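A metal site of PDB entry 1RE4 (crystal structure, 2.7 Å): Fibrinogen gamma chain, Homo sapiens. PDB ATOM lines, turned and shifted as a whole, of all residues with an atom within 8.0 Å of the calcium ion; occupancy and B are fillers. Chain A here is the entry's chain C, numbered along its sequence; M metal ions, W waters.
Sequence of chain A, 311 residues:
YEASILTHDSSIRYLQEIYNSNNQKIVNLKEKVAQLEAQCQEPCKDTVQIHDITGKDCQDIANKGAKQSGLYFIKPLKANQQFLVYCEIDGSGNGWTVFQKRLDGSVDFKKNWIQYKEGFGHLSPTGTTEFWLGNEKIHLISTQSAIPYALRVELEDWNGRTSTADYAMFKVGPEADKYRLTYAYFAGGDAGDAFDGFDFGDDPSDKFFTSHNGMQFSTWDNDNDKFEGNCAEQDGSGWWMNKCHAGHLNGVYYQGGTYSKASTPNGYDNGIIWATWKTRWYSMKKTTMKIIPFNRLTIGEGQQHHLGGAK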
ATOM      1  N   SER A 218     -18.850   6.903   4.234  1.00  0.00           N
ATOM      2  CA  SER A 218     -18.814   8.366   4.108  1.00  0.00           C
ATOM      3  C   SER A 218     -20.153   9.027   4.381  1.00  0.00           C
ATOM      4  O   SER A 218     -21.212   8.444   4.155  1.00  0.00           O
ATOM      5  CB  SER A 218     -18.354   8.763   2.691  1.00  0.00           C
ATOM      6  OG  SER A 218     -16.977   8.498   2.495  1.00  0.00           O
ATOM      7  N   ASN A 222     -18.064  14.012   6.688  1.00  0.00           N
ATOM      8  CA  ASN A 222     -16.907  13.152   6.901  1.00  0.00           C
ATOM      9  C   ASN A 222     -16.564  12.423   5.612  1.00  0.00           C
ATOM     10  O   ASN A 222     -16.865  11.252   5.446  1.00  0.00           O
ATOM     11  CB  ASN A 222     -17.207  12.156   8.031  1.00  0.00           C
ATOM     12  CG  ASN A 222     -15.948  11.598   8.673  1.00  0.00           C
ATOM     13  OD1 ASN A 222     -15.966  11.201   9.840  1.00  0.00           O
ATOM     14  ND2 ASN A 222     -14.863  11.550   7.928  1.00  0.00           N
ATOM     15  N   ASP A 223     -15.918  13.145   4.696  1.00  0.00           N
ATOM     16  CA  ASP A 223     -15.538  12.625   3.392  1.00  0.00           C
ATOM     17  C   ASP A 223     -14.433  11.582   3.452  1.00  0.00           C
ATOM     18  O   ASP A 223     -13.316  11.862   3.903  1.00  0.00           O
ATOM     19  CB  ASP A 223     -15.100  13.772   2.469  1.00  0.00           C
ATOM     20  CG  ASP A 223     -15.017  13.370   1.003  1.00  0.00           C
ATOM     21  OD1 ASP A 223     -14.303  12.391   0.689  1.00  0.00           O
ATOM     22  OD2 ASP A 223     -15.673  14.021   0.168  1.00  0.00           O
ATOM     23  N   ASN A 224     -14.737  10.362   3.001  1.00  0.00           N
ATOM     24  CA  ASN A 224     -13.747   9.288   2.996  1.00  0.00           C
ATOM     25  C   ASN A 224     -13.807   8.549   1.666  1.00  0.00           C
ATOM     26  O   ASN A 224     -13.274   7.459   1.532  1.00  0.00           O
ATOM     27  CB  ASN A 224     -14.004   8.310   4.151  1.00  0.00           C
ATOM     28  CG  ASN A 224     -13.644   8.900   5.518  1.00  0.00           C
ATOM     29  OD1 ASN A 224     -14.488   9.009   6.398  1.00  0.00           O
ATOM     30  ND2 ASN A 224     -12.379   9.284   5.691  1.00  0.00           N
ATOM     31  N   ASP A 225     -14.452   9.168   0.682  1.00  0.00           N
ATOM     32  CA  ASP A 225     -14.585   8.560  -0.641  1.00  0.00           C
ATOM     33  C   ASP A 225     -13.317   8.689  -1.491  1.00  0.00           C
ATOM     34  O   ASP A 225     -12.368   9.364  -1.109  1.00  0.00           O
ATOM     35  CB  ASP A 225     -15.751   9.212  -1.391  1.00  0.00           C
ATOM     36  CG  ASP A 225     -15.573  10.715  -1.574  1.00  0.00           C
ATOM     37  OD1 ASP A 225     -14.415  11.182  -1.676  1.00  0.00           O
ATOM     38  OD2 ASP A 225     -16.584  11.438  -1.635  1.00  0.00           O
ATOM     39  N   LYS A 226     -13.332   8.030  -2.644  1.00  0.00           N
ATOM     40  CA  LYS A 226     -12.210   8.069  -3.586  1.00  0.00           C
ATOM     41  C   LYS A 226     -12.462   9.138  -4.659  1.00  0.00           C
ATOM     42  O   LYS A 226     -12.022   8.993  -5.806  1.00  0.00           O
ATOM     43  CB  LYS A 226     -12.041   6.706  -4.276  1.00  0.00           C
ATOM     44  CG  LYS A 226     -11.743   5.556  -3.331  1.00  0.00           C
ATOM     45  CD  LYS A 226     -10.384   5.716  -2.686  1.00  0.00           C
ATOM     46  CE  LYS A 226     -10.158   4.639  -1.628  1.00  0.00           C
ATOM     47  NZ  LYS A 226      -8.824   4.769  -0.968  1.00  0.00           N
ATOM     48  N   PHE A 227     -13.174  10.186  -4.288  1.00  0.00           N
ATOM     49  CA  PHE A 227     -13.507  11.278  -5.208  1.00  0.00           C
ATOM     50  C   PHE A 227     -12.969  12.604  -4.660  1.00  0.00           C
ATOM     51  O   PHE A 227     -13.074  12.886  -3.474  1.00  0.00           O
ATOM     52  CB  PHE A 227     -15.032  11.320  -5.403  1.00  0.00           C
ATOM     53  CG  PHE A 227     -15.512  12.444  -6.292  1.00  0.00           C
ATOM     54  CD1 PHE A 227     -14.720  12.944  -7.313  1.00  0.00           C
ATOM     55  CD2 PHE A 227     -16.785  12.975  -6.109  1.00  0.00           C
ATOM     56  CE1 PHE A 227     -15.186  13.957  -8.155  1.00  0.00           C
ATOM     57  CE2 PHE A 227     -17.270  13.997  -6.945  1.00  0.00           C
ATOM     58  CZ  PHE A 227     -16.468  14.484  -7.962  1.00  0.00           C
ATOM     59  N   GLU A 228     -12.393  13.422  -5.542  1.00  0.00           N
ATOM     60  CA  GLU A 228     -11.826  14.707  -5.150  1.00  0.00           C
ATOM     61  C   GLU A 228     -12.913  15.587  -4.545  1.00  0.00           C
ATOM     62  O   GLU A 228     -12.624  16.594  -3.907  1.00  0.00           O
ATOM     63  CB  GLU A 228     -11.235  15.425  -6.369  1.00  0.00           C
ATOM     64  CG  GLU A 228     -10.376  14.562  -7.292  1.00  0.00           C
ATOM     65  CD  GLU A 228     -11.188  13.838  -8.381  1.00  0.00           C
ATOM     66  OE1 GLU A 228     -11.745  12.763  -8.099  1.00  0.00           O
ATOM     67  OE2 GLU A 228     -11.256  14.372  -9.511  1.00  0.00           O
ATOM     68  N   GLY A 229     -14.164  15.201  -4.764  1.00  0.00           N
ATOM     69  CA  GLY A 229     -15.279  15.941  -4.217  1.00  0.00           C
ATOM     70  C   GLY A 229     -15.940  15.154  -3.115  1.00  0.00           C
ATOM     71  O   GLY A 229     -15.312  14.282  -2.507  1.00  0.00           O
ATOM     72  N   ASN A 230     -17.214  15.432  -2.855  1.00  0.00           N
ATOM     73  CA  ASN A 230     -17.929  14.748  -1.799  1.00  0.00           C
ATOM     74  C   ASN A 230     -19.107  13.917  -2.282  1.00  0.00           C
ATOM     75  O   ASN A 230     -20.168  14.460  -2.573  1.00  0.00           O
ATOM     76  CB  ASN A 230     -18.410  15.762  -0.763  1.00  0.00           C
ATOM     77  CG  ASN A 230     -19.019  15.121   0.461  1.00  0.00           C
ATOM     78  OD1 ASN A 230     -18.956  15.683   1.559  1.00  0.00           O
ATOM     79  ND2 ASN A 230     -19.625  13.957   0.296  1.00  0.00           N
ATOM     80  N   CYS A 231     -18.909  12.608  -2.351  1.00  0.00           N
ATOM     81  CA  CYS A 231     -19.970  11.705  -2.800  1.00  0.00           C
ATOM     82  C   CYS A 231     -21.183  11.770  -1.877  1.00  0.00           C
ATOM     83  O   CYS A 231     -22.261  12.184  -2.301  1.00  0.00           O
ATOM     84  CB  CYS A 231     -19.451  10.263  -2.886  1.00  0.00           C
ATOM     85  SG  CYS A 231     -18.347   9.880  -4.308  1.00  0.00           S
ATOM     86  N   ALA A 232     -21.007  11.349  -0.629  1.00  0.00           N
ATOM     87  CA  ALA A 232     -22.086  11.346   0.354  1.00  0.00           C
ATOM     88  C   ALA A 232     -22.908  12.635   0.333  1.00  0.00           C
ATOM     89  O   ALA A 232     -24.137  12.600   0.482  1.00  0.00           O
ATOM     90  CB  ALA A 232     -21.519  11.131   1.747  1.00  0.00           C
ATOM     91  N   ASN A 242     -17.204   5.453  -3.386  1.00  0.00           N
ATOM     92  CA  ASN A 242     -15.963   5.277  -4.113  1.00  0.00           C
ATOM     93  C   ASN A 242     -15.805   6.503  -5.004  1.00  0.00           C
ATOM     94  O   ASN A 242     -15.037   7.404  -4.674  1.00  0.00           O
ATOM     95  CB  ASN A 242     -16.037   3.989  -4.965  1.00  0.00           C
ATOM     96  CG  ASN A 242     -14.734   3.651  -5.671  1.00  0.00           C
ATOM     97  OD1 ASN A 242     -14.565   2.557  -6.180  1.00  0.00           O
ATOM     98  ND2 ASN A 242     -13.807   4.601  -5.691  1.00  0.00           N
HETATM   99 CA    CA M   1     -13.567  13.355  -1.430  1.00  0.00          CA
HETATM  100  O   HOH W   1     -12.029  12.039  -0.341  1.00  0.00           O
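The side-chain hydroxyl (OG) of Ser 218 is in hydrogen-bond range of the backbone NH (N) of Asp 225 (3.2 Å).
N of Phe 227 lies within hydrogen-bond range of O of Asn 242 (3.4 Å).
N of Cys 231 is in hydrogen-bond range of OD2 of Asp 225, at 2.7 Å.
Residues that only touch the calcium ion: Glu 228 (3.9 Å).
Within 4 Å of the calcium ion: Asp 223, Asp 225, Phe 227, Glu 228 and Gly 229.
The nearest printed residue that does not touch the calcium ion is Asn 230 (4.4 Å).
The calcium ion is bound by the backbone carbonyl oxygen (O) of Phe 227, at 2.2 Å.
O of Gly 229 binds the calcium ion, 2.3 Å away.
The calcium ion is bound by water W1.
OD1 of Asp 225 is bound to the calcium ion (2.3 Å).
OD1 of Asp 223 binds the calcium ion.
OD2 of Asp 223 binds the calcium ion, 2.7 Å away.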
